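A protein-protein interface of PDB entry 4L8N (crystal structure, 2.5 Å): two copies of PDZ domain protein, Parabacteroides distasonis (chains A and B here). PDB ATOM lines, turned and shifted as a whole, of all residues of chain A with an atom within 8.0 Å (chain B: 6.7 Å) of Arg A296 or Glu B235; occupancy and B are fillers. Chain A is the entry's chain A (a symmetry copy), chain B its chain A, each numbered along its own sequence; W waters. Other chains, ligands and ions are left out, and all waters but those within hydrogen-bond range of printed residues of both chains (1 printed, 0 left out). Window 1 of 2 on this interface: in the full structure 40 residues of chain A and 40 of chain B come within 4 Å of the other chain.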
ATOM      1  N   VAL A 128     -14.655  21.473  20.643  1.00  0.00           N
ATOM      2  CA  VAL A 128     -13.665  21.469  21.709  1.00  0.00           C
ATOM      3  C   VAL A 128     -12.562  22.451  21.323  1.00  0.00           C
ATOM      4  O   VAL A 128     -12.151  22.476  20.155  1.00  0.00           O
ATOM      5  CB  VAL A 128     -13.119  20.043  22.021  1.00  0.00           C
ATOM      6  CG1 VAL A 128     -12.296  20.058  23.293  1.00  0.00           C
ATOM      7  CG2 VAL A 128     -14.250  19.028  22.163  1.00  0.00           C
ATOM      8  N   CYS A 129     -12.110  23.284  22.301  1.00  0.00           N
ATOM      9  CA  CYS A 129     -11.056  24.285  22.066  1.00  0.00           C
ATOM     10  C   CYS A 129      -9.762  23.919  22.774  1.00  0.00           C
ATOM     11  O   CYS A 129      -9.774  23.411  23.908  1.00  0.00           O
ATOM     12  CB  CYS A 129     -11.524  25.674  22.470  1.00  0.00           C
ATOM     13  SG  CYS A 129     -12.845  26.331  21.431  1.00  0.00           S
ATOM     14  N   PRO A 130      -8.614  24.200  22.121  1.00  0.00           N
ATOM     15  CA  PRO A 130      -7.325  23.846  22.735  1.00  0.00           C
ATOM     16  C   PRO A 130      -6.888  24.966  23.659  1.00  0.00           C
ATOM     17  O   PRO A 130      -5.940  25.707  23.380  1.00  0.00           O
ATOM     18  CB  PRO A 130      -6.408  23.641  21.522  1.00  0.00           C
ATOM     19  CG  PRO A 130      -6.960  24.564  20.490  1.00  0.00           C
ATOM     20  CD  PRO A 130      -8.414  24.841  20.802  1.00  0.00           C
ATOM     21  N   PHE A 131      -7.644  25.122  24.745  1.00  0.00           N
ATOM     22  CA  PHE A 131      -7.359  26.148  25.737  1.00  0.00           C
ATOM     23  C   PHE A 131      -6.764  25.518  26.979  1.00  0.00           C
ATOM     24  O   PHE A 131      -7.367  24.604  27.540  1.00  0.00           O
ATOM     25  CB  PHE A 131      -8.645  26.931  26.125  1.00  0.00           C
ATOM     26  CG  PHE A 131      -9.391  27.679  25.040  1.00  0.00           C
ATOM     27  CD1 PHE A 131      -8.745  28.078  23.869  1.00  0.00           C
ATOM     28  CD2 PHE A 131     -10.733  28.029  25.210  1.00  0.00           C
ATOM     29  CE1 PHE A 131      -9.434  28.781  22.871  1.00  0.00           C
ATOM     30  CE2 PHE A 131     -11.416  28.741  24.219  1.00  0.00           C
ATOM     31  CZ  PHE A 131     -10.766  29.109  23.053  1.00  0.00           C
ATOM     32  N   LYS A 132      -5.611  26.008  27.424  1.00  0.00           N
ATOM     33  CA  LYS A 132      -5.042  25.585  28.693  1.00  0.00           C
ATOM     34  C   LYS A 132      -5.417  26.702  29.686  1.00  0.00           C
ATOM     35  O   LYS A 132      -5.010  27.859  29.500  1.00  0.00           O
ATOM     36  CB  LYS A 132      -3.515  25.314  28.600  1.00  0.00           C
ATOM     37  CG  LYS A 132      -2.803  25.064  29.945  1.00  0.00           C
ATOM     38  CD  LYS A 132      -3.019  23.640  30.490  1.00  0.00           C
ATOM     39  CE  LYS A 132      -2.598  23.528  31.940  1.00  0.00           C
ATOM     40  NZ  LYS A 132      -3.656  23.972  32.900  1.00  0.00           N
ATOM     41  N   THR A 133      -6.259  26.363  30.688  1.00  0.00           N
ATOM     42  CA  THR A 133      -6.735  27.327  31.693  1.00  0.00           C
ATOM     43  C   THR A 133      -6.184  26.894  33.020  1.00  0.00           C
ATOM     44  O   THR A 133      -6.458  25.782  33.483  1.00  0.00           O
ATOM     45  CB  THR A 133      -8.284  27.481  31.669  1.00  0.00           C
ATOM     46  OG1 THR A 133      -8.669  27.604  30.307  1.00  0.00           O
ATOM     47  CG2 THR A 133      -8.762  28.732  32.390  1.00  0.00           C
ATOM     48  N   THR A 134      -5.357  27.776  33.602  1.00  0.00           N
ATOM     49  CA  THR A 134      -4.618  27.578  34.846  1.00  0.00           C
ATOM     50  C   THR A 134      -4.938  28.679  35.818  1.00  0.00           C
ATOM     51  O   THR A 134      -4.914  29.856  35.456  1.00  0.00           O
ATOM     52  CB  THR A 134      -3.115  27.559  34.564  1.00  0.00           C
ATOM     53  OG1 THR A 134      -2.844  26.841  33.356  1.00  0.00           O
ATOM     54  CG2 THR A 134      -2.312  26.990  35.726  1.00  0.00           C
ATOM     55  N   LEU A 229       1.133   7.734  24.151  1.00  0.00           N
ATOM     56  CA  LEU A 229       0.815   7.974  22.750  1.00  0.00           C
ATOM     57  C   LEU A 229       1.745   9.031  22.161  1.00  0.00           C
ATOM     58  O   LEU A 229       1.779  10.169  22.648  1.00  0.00           O
ATOM     59  CB  LEU A 229      -0.662   8.398  22.584  1.00  0.00           C
ATOM     60  CG  LEU A 229      -1.744   7.322  22.742  1.00  0.00           C
ATOM     61  CD1 LEU A 229      -3.121   7.954  22.726  1.00  0.00           C
ATOM     62  CD2 LEU A 229      -1.700   6.336  21.605  1.00  0.00           C
ATOM     63  N   TYR A 231       2.081  11.365  19.520  1.00  0.00           N
ATOM     64  CA  TYR A 231       1.301  12.188  18.584  1.00  0.00           C
ATOM     65  C   TYR A 231       2.174  13.088  17.658  1.00  0.00           C
ATOM     66  O   TYR A 231       1.611  13.786  16.806  1.00  0.00           O
ATOM     67  CB  TYR A 231       0.327  13.073  19.383  1.00  0.00           C
ATOM     68  N   GLU A 263      -4.435  30.008  27.858  1.00  0.00           N
ATOM     69  CA  GLU A 263      -3.536  29.937  26.713  1.00  0.00           C
ATOM     70  C   GLU A 263      -4.101  29.010  25.656  1.00  0.00           C
ATOM     71  O   GLU A 263      -4.422  27.861  25.928  1.00  0.00           O
ATOM     72  CB  GLU A 263      -2.140  29.454  27.160  1.00  0.00           C
ATOM     73  CG  GLU A 263      -1.014  29.751  26.189  1.00  0.00           C
ATOM     74  CD  GLU A 263       0.317  29.131  26.557  1.00  0.00           C
ATOM     75  OE1 GLU A 263       0.922  29.550  27.571  1.00  0.00           O
ATOM     76  OE2 GLU A 263       0.778  28.247  25.804  1.00  0.00           O
ATOM     77  N   GLN A 288     -14.690  30.920  31.027  1.00  0.00           N
ATOM     78  CA  GLN A 288     -14.198  30.244  32.214  1.00  0.00           C
ATOM     79  C   GLN A 288     -13.684  31.229  33.258  1.00  0.00           C
ATOM     80  O   GLN A 288     -13.141  30.789  34.261  1.00  0.00           O
ATOM     81  CB  GLN A 288     -13.174  29.162  31.888  1.00  0.00           C
ATOM     82  CG  GLN A 288     -13.852  27.944  31.281  1.00  0.00           C
ATOM     83  CD  GLN A 288     -13.094  26.698  31.536  1.00  0.00           C
ATOM     84  OE1 GLN A 288     -13.522  25.831  32.304  1.00  0.00           O
ATOM     85  NE2 GLN A 288     -11.930  26.607  30.916  1.00  0.00           N
ATOM     86  N   THR A 292     -14.050  28.327  36.307  1.00  0.00           N
ATOM     87  CA  THR A 292     -13.179  27.398  35.600  1.00  0.00           C
ATOM     88  C   THR A 292     -13.454  25.966  36.067  1.00  0.00           C
ATOM     89  O   THR A 292     -13.259  25.654  37.246  1.00  0.00           O
ATOM     90  CB  THR A 292     -11.693  27.788  35.830  1.00  0.00           C
ATOM     91  OG1 THR A 292     -11.441  29.108  35.346  1.00  0.00           O
ATOM     92  CG2 THR A 292     -10.717  26.837  35.162  1.00  0.00           C
ATOM     93  N   LYS A 293     -13.899  25.089  35.142  1.00  0.00           N
ATOM     94  CA  LYS A 293     -14.076  23.683  35.475  1.00  0.00           C
ATOM     95  C   LYS A 293     -13.236  22.762  34.538  1.00  0.00           C
ATOM     96  O   LYS A 293     -12.953  21.633  34.925  1.00  0.00           O
ATOM     97  CB  LYS A 293     -15.546  23.243  35.589  1.00  0.00           C
ATOM     98  CG  LYS A 293     -16.477  23.452  34.412  1.00  0.00           C
ATOM     99  CD  LYS A 293     -17.785  22.679  34.679  1.00  0.00           C
ATOM    100  CE  LYS A 293     -18.901  23.053  33.729  1.00  0.00           C
ATOM    101  NZ  LYS A 293     -19.969  22.014  33.694  1.00  0.00           N
ATOM    102  N   TYR A 294     -12.749  23.265  33.388  1.00  0.00           N
ATOM    103  CA  TYR A 294     -11.890  22.511  32.448  1.00  0.00           C
ATOM    104  C   TYR A 294     -10.514  23.138  32.328  1.00  0.00           C
ATOM    105  O   TYR A 294     -10.390  24.267  31.867  1.00  0.00           O
ATOM    106  CB  TYR A 294     -12.525  22.408  31.052  1.00  0.00           C
ATOM    107  CG  TYR A 294     -13.825  21.646  31.093  1.00  0.00           C
ATOM    108  CD1 TYR A 294     -13.837  20.259  31.206  1.00  0.00           C
ATOM    109  CD2 TYR A 294     -15.044  22.313  31.129  1.00  0.00           C
ATOM    110  CE1 TYR A 294     -15.030  19.555  31.323  1.00  0.00           C
ATOM    111  CE2 TYR A 294     -16.244  21.616  31.234  1.00  0.00           C
ATOM    112  CZ  TYR A 294     -16.231  20.236  31.323  1.00  0.00           C
ATOM    113  OH  TYR A 294     -17.403  19.529  31.427  1.00  0.00           O
ATOM    114  N   GLY A 295      -9.492  22.388  32.706  1.00  0.00           N
ATOM    115  CA  GLY A 295      -8.123  22.874  32.638  1.00  0.00           C
ATOM    116  C   GLY A 295      -7.427  22.746  31.301  1.00  0.00           C
ATOM    117  O   GLY A 295      -6.553  23.556  30.993  1.00  0.00           O
ATOM    118  N   ARG A 296      -7.775  21.727  30.499  1.00  0.00           N
ATOM    119  CA  ARG A 296      -7.011  21.504  29.267  1.00  0.00           C
ATOM    120  C   ARG A 296      -7.775  21.547  27.932  1.00  0.00           C
ATOM    121  O   ARG A 296      -7.197  22.065  26.972  1.00  0.00           O
ATOM    122  CB  ARG A 296      -6.221  20.187  29.342  1.00  0.00           C
ATOM    123  CG  ARG A 296      -4.772  20.378  28.900  1.00  0.00           C
ATOM    124  CD  ARG A 296      -3.913  19.144  29.080  1.00  0.00           C
ATOM    125  NE  ARG A 296      -4.303  18.049  28.185  1.00  0.00           N
ATOM    126  CZ  ARG A 296      -3.826  17.875  26.956  1.00  0.00           C
ATOM    127  NH1 ARG A 296      -2.944  18.730  26.451  1.00  0.00           N
ATOM    128  NH2 ARG A 296      -4.232  16.847  26.221  1.00  0.00           N
ATOM    129  N   ASN A 297      -8.953  20.946  27.796  1.00  0.00           N
ATOM    130  CA  ASN A 297      -9.625  20.977  26.478  1.00  0.00           C
ATOM    131  C   ASN A 297     -11.054  21.307  26.741  1.00  0.00           C
ATOM    132  O   ASN A 297     -11.754  20.453  27.305  1.00  0.00           O
ATOM    133  CB  ASN A 297      -9.479  19.641  25.713  1.00  0.00           C
ATOM    134  CG  ASN A 297      -8.074  19.262  25.289  1.00  0.00           C
ATOM    135  OD1 ASN A 297      -7.532  18.245  25.729  1.00  0.00           O
ATOM    136  ND2 ASN A 297      -7.452  20.039  24.399  1.00  0.00           N
ATOM    137  N   VAL A 298     -11.482  22.558  26.415  1.00  0.00           N
ATOM    138  CA  VAL A 298     -12.818  23.034  26.771  1.00  0.00           C
ATOM    139  C   VAL A 298     -13.919  22.562  25.801  1.00  0.00           C
ATOM    140  O   VAL A 298     -13.987  23.016  24.645  1.00  0.00           O
ATOM    141  CB  VAL A 298     -12.925  24.577  26.987  1.00  0.00           C
ATOM    142  CG1 VAL A 298     -14.185  24.927  27.778  1.00  0.00           C
ATOM    143  CG2 VAL A 298     -11.684  25.151  27.664  1.00  0.00           C
ATOM    144  N   PRO A 299     -14.882  21.782  26.350  1.00  0.00           N
ATOM    145  CA  PRO A 299     -16.047  21.372  25.560  1.00  0.00           C
ATOM    146  C   PRO A 299     -17.181  22.426  25.572  1.00  0.00           C
ATOM    147  O   PRO A 299     -17.629  22.858  26.651  1.00  0.00           O
ATOM    148  CB  PRO A 299     -16.485  20.086  26.268  1.00  0.00           C
ATOM    149  CG  PRO A 299     -16.149  20.298  27.683  1.00  0.00           C
ATOM    150  CD  PRO A 299     -14.953  21.223  27.719  1.00  0.00           C
ATOM    151  N   ASN B 197      -9.799   8.461  30.530  1.00  0.00           N
ATOM    152  CA  ASN B 197     -10.203   9.501  29.600  1.00  0.00           C
ATOM    153  C   ASN B 197     -11.715   9.340  29.294  1.00  0.00           C
ATOM    154  O   ASN B 197     -12.120   8.278  28.798  1.00  0.00           O
ATOM    155  CB  ASN B 197      -9.352   9.417  28.323  1.00  0.00           C
ATOM    156  CG  ASN B 197      -9.758  10.298  27.144  1.00  0.00           C
ATOM    157  OD1 ASN B 197     -10.537  11.253  27.250  1.00  0.00           O
ATOM    158  ND2 ASN B 197      -9.211  10.002  25.976  1.00  0.00           N
ATOM    159  N   ASN B 199     -13.370  10.715  26.877  1.00  0.00           N
ATOM    160  CA  ASN B 199     -13.396  10.658  25.407  1.00  0.00           C
ATOM    161  C   ASN B 199     -12.903   9.287  24.825  1.00  0.00           C
ATOM    162  O   ASN B 199     -12.787   9.178  23.601  1.00  0.00           O
ATOM    163  CB  ASN B 199     -12.579  11.813  24.808  1.00  0.00           C
ATOM    164  N   TYR B 200     -12.644   8.249  25.677  1.00  0.00           N
ATOM    165  CA  TYR B 200     -12.249   6.908  25.213  1.00  0.00           C
ATOM    166  C   TYR B 200     -13.509   6.097  24.869  1.00  0.00           C
ATOM    167  O   TYR B 200     -14.384   5.925  25.729  1.00  0.00           O
ATOM    168  CB  TYR B 200     -11.392   6.168  26.249  1.00  0.00           C
ATOM    169  CG  TYR B 200     -10.832   4.857  25.737  1.00  0.00           C
ATOM    170  CD1 TYR B 200      -9.982   4.820  24.636  1.00  0.00           C
ATOM    171  CD2 TYR B 200     -11.114   3.656  26.383  1.00  0.00           C
ATOM    172  CE1 TYR B 200      -9.454   3.619  24.164  1.00  0.00           C
ATOM    173  CE2 TYR B 200     -10.588   2.446  25.923  1.00  0.00           C
ATOM    174  CZ  TYR B 200      -9.761   2.433  24.809  1.00  0.00           C
ATOM    175  OH  TYR B 200      -9.198   1.261  24.356  1.00  0.00           O
ATOM    176  N   TYR B 231      -7.217  17.619  16.039  1.00  0.00           N
ATOM    177  CA  TYR B 231      -6.526  16.425  16.548  1.00  0.00           C
ATOM    178  C   TYR B 231      -7.391  15.564  17.519  1.00  0.00           C
ATOM    179  O   TYR B 231      -6.912  14.515  17.967  1.00  0.00           O
ATOM    180  CB  TYR B 231      -5.234  16.857  17.263  1.00  0.00           C
ATOM    181  N   ALA B 232      -8.657  15.990  17.813  1.00  0.00           N
ATOM    182  CA  ALA B 232      -9.626  15.369  18.743  1.00  0.00           C
ATOM    183  C   ALA B 232      -9.806  13.829  18.588  1.00  0.00           C
ATOM    184  O   ALA B 232     -10.223  13.176  19.552  1.00  0.00           O
ATOM    185  CB  ALA B 232     -10.980  16.049  18.610  1.00  0.00           C
ATOM    186  N   ALA B 233      -9.500  13.268  17.393  1.00  0.00           N
ATOM    187  CA  ALA B 233      -9.587  11.835  17.091  1.00  0.00           C
ATOM    188  C   ALA B 233      -8.435  11.040  17.760  1.00  0.00           C
ATOM    189  O   ALA B 233      -8.662   9.918  18.214  1.00  0.00           O
ATOM    190  CB  ALA B 233      -9.574  11.622  15.585  1.00  0.00           C
ATOM    191  N   ALA B 234      -7.220  11.626  17.836  1.00  0.00           N
ATOM    192  CA  ALA B 234      -6.042  11.011  18.479  1.00  0.00           C
ATOM    193  C   ALA B 234      -6.188  10.990  20.014  1.00  0.00           C
ATOM    194  O   ALA B 234      -5.606  10.126  20.675  1.00  0.00           O
ATOM    195  CB  ALA B 234      -4.775  11.755  18.084  1.00  0.00           C
ATOM    196  N   GLU B 235      -6.964  11.952  20.567  1.00  0.00           N
ATOM    197  CA  GLU B 235      -7.266  12.083  21.994  1.00  0.00           C
ATOM    198  C   GLU B 235      -8.136  10.922  22.455  1.00  0.00           C
ATOM    199  O   GLU B 235      -7.943  10.416  23.561  1.00  0.00           O
ATOM    200  CB  GLU B 235      -7.977  13.417  22.279  1.00  0.00           C
ATOM    201  CG  GLU B 235      -7.041  14.605  22.449  1.00  0.00           C
ATOM    202  CD  GLU B 235      -6.786  15.090  23.868  1.00  0.00           C
ATOM    203  OE1 GLU B 235      -7.604  14.784  24.768  1.00  0.00           O
ATOM    204  OE2 GLU B 235      -5.782  15.816  24.068  1.00  0.00           O
ATOM    205  N   ALA B 236      -9.086  10.496  21.593  1.00  0.00           N
ATOM    206  CA  ALA B 236     -10.012   9.385  21.825  1.00  0.00           C
ATOM    207  C   ALA B 236      -9.284   8.021  21.945  1.00  0.00           C
ATOM    208  O   ALA B 236      -9.794   7.115  22.600  1.00  0.00           O
ATOM    209  CB  ALA B 236     -11.035   9.330  20.701  1.00  0.00           C
ATOM    210  N   GLU B 237      -8.098   7.893  21.324  1.00  0.00           N
ATOM    211  CA  GLU B 237      -7.260   6.683  21.333  1.00  0.00           C
ATOM    212  C   GLU B 237      -6.713   6.336  22.741  1.00  0.00           C
ATOM    213  O   GLU B 237      -6.363   5.173  22.988  1.00  0.00           O
ATOM    214  CB  GLU B 237      -6.074   6.836  20.352  1.00  0.00           C
ATOM    215  CG  GLU B 237      -6.464   7.170  18.917  1.00  0.00           C
ATOM    216  CD  GLU B 237      -7.230   6.093  18.169  1.00  0.00           C
ATOM    217  OE1 GLU B 237      -6.713   4.958  18.054  1.00  0.00           O
ATOM    218  OE2 GLU B 237      -8.343   6.393  17.679  1.00  0.00           O
ATOM    219  N   ALA B 238      -6.639   7.342  23.648  1.00  0.00           N
ATOM    220  CA  ALA B 238      -6.123   7.199  25.011  1.00  0.00           C
ATOM    221  C   ALA B 238      -7.202   6.770  26.012  1.00  0.00           C
ATOM    222  O   ALA B 238      -8.207   7.462  26.152  1.00  0.00           O
ATOM    223  CB  ALA B 238      -5.502   8.511  25.466  1.00  0.00           C
ATOM    224  N   GLU B 239      -6.967   5.660  26.743  1.00  0.00           N
ATOM    225  CA  GLU B 239      -7.894   5.185  27.786  1.00  0.00           C
ATOM    226  C   GLU B 239      -7.739   6.024  29.022  1.00  0.00           C
ATOM    227  O   GLU B 239      -8.727   6.348  29.666  1.00  0.00           O
ATOM    228  CB  GLU B 239      -7.675   3.698  28.177  1.00  0.00           C
ATOM    229  CG  GLU B 239      -7.162   2.755  27.096  1.00  0.00           C
ATOM    230  CD  GLU B 239      -7.159   1.272  27.436  1.00  0.00           C
ATOM    231  OE1 GLU B 239      -7.690   0.890  28.505  1.00  0.00           O
ATOM    232  OE2 GLU B 239      -6.611   0.489  26.625  1.00  0.00           O
ATOM    233  N   LEU B 241      -5.457   9.301  31.275  1.00  0.00           N
ATOM    234  CA  LEU B 241      -4.829  10.624  31.237  1.00  0.00           C
ATOM    235  C   LEU B 241      -3.903  10.778  32.429  1.00  0.00           C
ATOM    236  O   LEU B 241      -4.257  10.399  33.560  1.00  0.00           O
ATOM    237  CB  LEU B 241      -5.870  11.769  31.209  1.00  0.00           C
ATOM    238  CG  LEU B 241      -6.920  11.711  30.103  1.00  0.00           C
ATOM    239  CD1 LEU B 241      -8.089  12.635  30.406  1.00  0.00           C
ATOM    240  CD2 LEU B 241      -6.319  11.949  28.720  1.00  0.00           C
ATOM    241  N   GLN B 243      -1.260  13.574  34.372  1.00  0.00           N
ATOM    242  CA  GLN B 243      -0.755  14.911  34.588  1.00  0.00           C
ATOM    243  C   GLN B 243       0.297  14.870  35.694  1.00  0.00           C
ATOM    244  O   GLN B 243       0.122  14.186  36.706  1.00  0.00           O
ATOM    245  CB  GLN B 243      -1.880  15.905  34.928  1.00  0.00           C
ATOM    246  CG  GLN B 243      -1.368  17.347  35.032  1.00  0.00           C
ATOM    247  CD  GLN B 243      -2.376  18.312  35.587  1.00  0.00           C
ATOM    248  OE1 GLN B 243      -2.953  19.114  34.852  1.00  0.00           O
ATOM    249  NE2 GLN B 243      -2.569  18.293  36.900  1.00  0.00           N
ATOM    250  N   GLU B 263       4.721  21.366  33.446  1.00  0.00           N
ATOM    251  CA  GLU B 263       3.584  20.454  33.460  1.00  0.00           C
ATOM    252  C   GLU B 263       3.685  19.467  32.316  1.00  0.00           C
ATOM    253  O   GLU B 263       3.820  19.847  31.161  1.00  0.00           O
ATOM    254  CB  GLU B 263       2.263  21.247  33.370  1.00  0.00           C
ATOM    255  CG  GLU B 263       1.025  20.490  33.813  1.00  0.00           C
ATOM    256  CD  GLU B 263      -0.280  21.216  33.566  1.00  0.00           C
ATOM    257  OE1 GLU B 263      -0.533  22.252  34.224  1.00  0.00           O
ATOM    258  OE2 GLU B 263      -1.074  20.723  32.737  1.00  0.00           O
ATOM    259  N   ASN B 265       1.729  16.465  30.357  1.00  0.00           N
ATOM    260  CA  ASN B 265       0.412  15.923  30.048  1.00  0.00           C
ATOM    261  C   ASN B 265       0.592  14.797  29.052  1.00  0.00           C
ATOM    262  O   ASN B 265       0.975  15.013  27.894  1.00  0.00           O
ATOM    263  CB  ASN B 265      -0.549  16.994  29.562  1.00  0.00           C
ATOM    264  CG  ASN B 265      -0.941  17.939  30.672  1.00  0.00           C
ATOM    265  OD1 ASN B 265      -1.724  17.588  31.572  1.00  0.00           O
ATOM    266  ND2 ASN B 265      -0.395  19.158  30.626  1.00  0.00           N
ATOM    267  N   GLU B 266       0.378  13.576  29.547  1.00  0.00           N
ATOM    268  CA  GLU B 266       0.616  12.337  28.819  1.00  0.00           C
ATOM    269  C   GLU B 266      -0.680  11.600  28.444  1.00  0.00           C
ATOM    270  O   GLU B 266      -1.569  11.465  29.283  1.00  0.00           O
ATOM    271  CB  GLU B 266       1.499  11.444  29.714  1.00  0.00           C
ATOM    272  CG  GLU B 266       2.530  10.634  28.968  1.00  0.00           C
ATOM    273  CD  GLU B 266       3.666  11.415  28.345  1.00  0.00           C
ATOM    274  OE1 GLU B 266       4.537  11.896  29.103  1.00  0.00           O
ATOM    275  OE2 GLU B 266       3.723  11.480  27.093  1.00  0.00           O
ATOM    276  N   LEU B 267      -0.790  11.147  27.177  1.00  0.00           N
ATOM    277  CA  LEU B 267      -1.952  10.353  26.703  1.00  0.00           C
ATOM    278  C   LEU B 267      -1.590   8.874  26.800  1.00  0.00           C
ATOM    279  O   LEU B 267      -0.707   8.394  26.079  1.00  0.00           O
ATOM    280  CB  LEU B 267      -2.407  10.716  25.274  1.00  0.00           C
ATOM    281  CG  LEU B 267      -3.048  12.087  25.053  1.00  0.00           C
ATOM    282  CD1 LEU B 267      -3.577  12.193  23.642  1.00  0.00           C
ATOM    283  CD2 LEU B 267      -4.183  12.343  26.014  1.00  0.00           C
ATOM    284  N   ARG B 296       6.830  24.562  24.958  1.00  0.00           N
ATOM    285  CA  ARG B 296       5.769  23.563  24.785  1.00  0.00           C
ATOM    286  C   ARG B 296       6.192  22.111  24.500  1.00  0.00           C
ATOM    287  O   ARG B 296       5.524  21.219  25.029  1.00  0.00           O
ATOM    288  CB  ARG B 296       4.768  24.007  23.706  1.00  0.00           C
ATOM    289  CG  ARG B 296       3.326  23.844  24.181  1.00  0.00           C
ATOM    290  CD  ARG B 296       2.300  24.390  23.209  1.00  0.00           C
ATOM    291  NE  ARG B 296       2.239  23.621  21.962  1.00  0.00           N
ATOM    292  CZ  ARG B 296       1.463  22.559  21.769  1.00  0.00           C
ATOM    293  NH1 ARG B 296       0.679  22.113  22.745  1.00  0.00           N
ATOM    294  NH2 ARG B 296       1.467  21.930  20.599  1.00  0.00           N
HETATM  295  O   HOH W   1       1.507  11.549  25.545  1.00  0.00           O
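OE2 of Glu B235 is in salt-bridge range of NH2 of Arg A296, at 2.8 Å.
The side-chain carboxylate (OE2) of Glu B235 sits close to the side-chain amide oxygen (OD1) of Asn A297.
The side-chain carboxylate of Glu B263 lies within salt-bridge range of the side-chain amino group of Lys A132.
The backbone carbonyl oxygen (O) of Leu B267 is in hydrogen-bond range of the backbone NH (N) of Leu A229.
Water W1 lies within hydrogen-bond range of the side-chain carboxylate of Glu B266, the backbone NH of Leu B267 and the backbone carbonyl oxygen of Leu A229.
Of the printed residues of chain B, Leu A229 touches Ala B234, Glu B237, Ala B238 and Leu B267.
Glu A263 touches none of the printed residues of chain B.
Of chain B, only Glu B235 and Asn B265 come within 4 Å of Arg A296.
Ala B232 touches none of the printed residues of chain A.
Of chain A, only Leu A229 (3.9 Å) comes within 4 Å of Ala B234.
Glu B235 touches just these residues of chain A: Arg A296 (2.8 Å) and Asn A297 (3.4 Å).
No residue of chain A comes within 4 Å of Ala B236.
Of the printed residues of chain A, Leu B267 touches Leu A229.
The nearest residue of chain B that does not touch Arg A296 is Leu B267 (4.5 Å).
The backbone carbonyl oxygen of Ala B238 sits at hydrogen-bond distance from the side-chain amide nitrogen of Asn B197 (2.7 Å).
The side-chain carboxylate of Glu B263 sits close to the side-chain amide oxygen of Gln B243, 3.3 Å away.
The side-chain carboxylate (OE2) of Glu B263 sits at hydrogen-bond distance from the side-chain amide nitrogen (ND2) of Asn B265.
The backbone carbonyl oxygen (O) of Phe A131 lies close to the backbone carbonyl oxygen (O) of Arg A296, at 2.6 Å.
The backbone carbonyl oxygen (O) of Glu A263 is in hydrogen-bond range of the backbone NH (N) of Lys A132 (2.7 Å).
The backbone carbonyl oxygen of Gly A295 sits close to the side-chain amino group of Lys A132, at 3.5 Å.
Printed residues of chain A that touch a printed residue of chain B: Lys A132, Leu A229, Arg A296 and Asn A297.
Hydrophobic or aromatic side chains of chain A within 4 Å of the printed part of chain B: Leu A229.
Of the 19 printed residues of chain B, 7 touch a printed residue of chain A.
Printed residues of chain B that touch a printed residue of chain A: Ala B234, Glu B235, Glu B237, Ala B238, Glu B263, Asn B265 and Leu B267.
Hydrophobic or aromatic side chains of chain B that line the printed part of chain A: Ala B238 and Leu B267.
Along chain B the printed residues that touch a printed residue of chain A span positions 234 to 267.
Among the printed residues, 8 pairs touch across the chains.
Among the printed residues, Asp or Glu carboxylates within 4 Å of a Lys or Arg side-chain nitrogen of the other chain: Lys A132 with Glu B263 (3.8 Å) and Arg A296 with Glu B235 (2.8 Å).
Positions printed for both chains: 231, 263 and 296.
Among the printed residues, pairs that only touch across the chains: Leu A229 with Ala B234 (3.9 Å), Leu A229 with Glu B237 (3.9 Å), Leu A229 with Ala B238 (3.7 Å) and Arg A296 with Asn B265 (3.6 Å).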
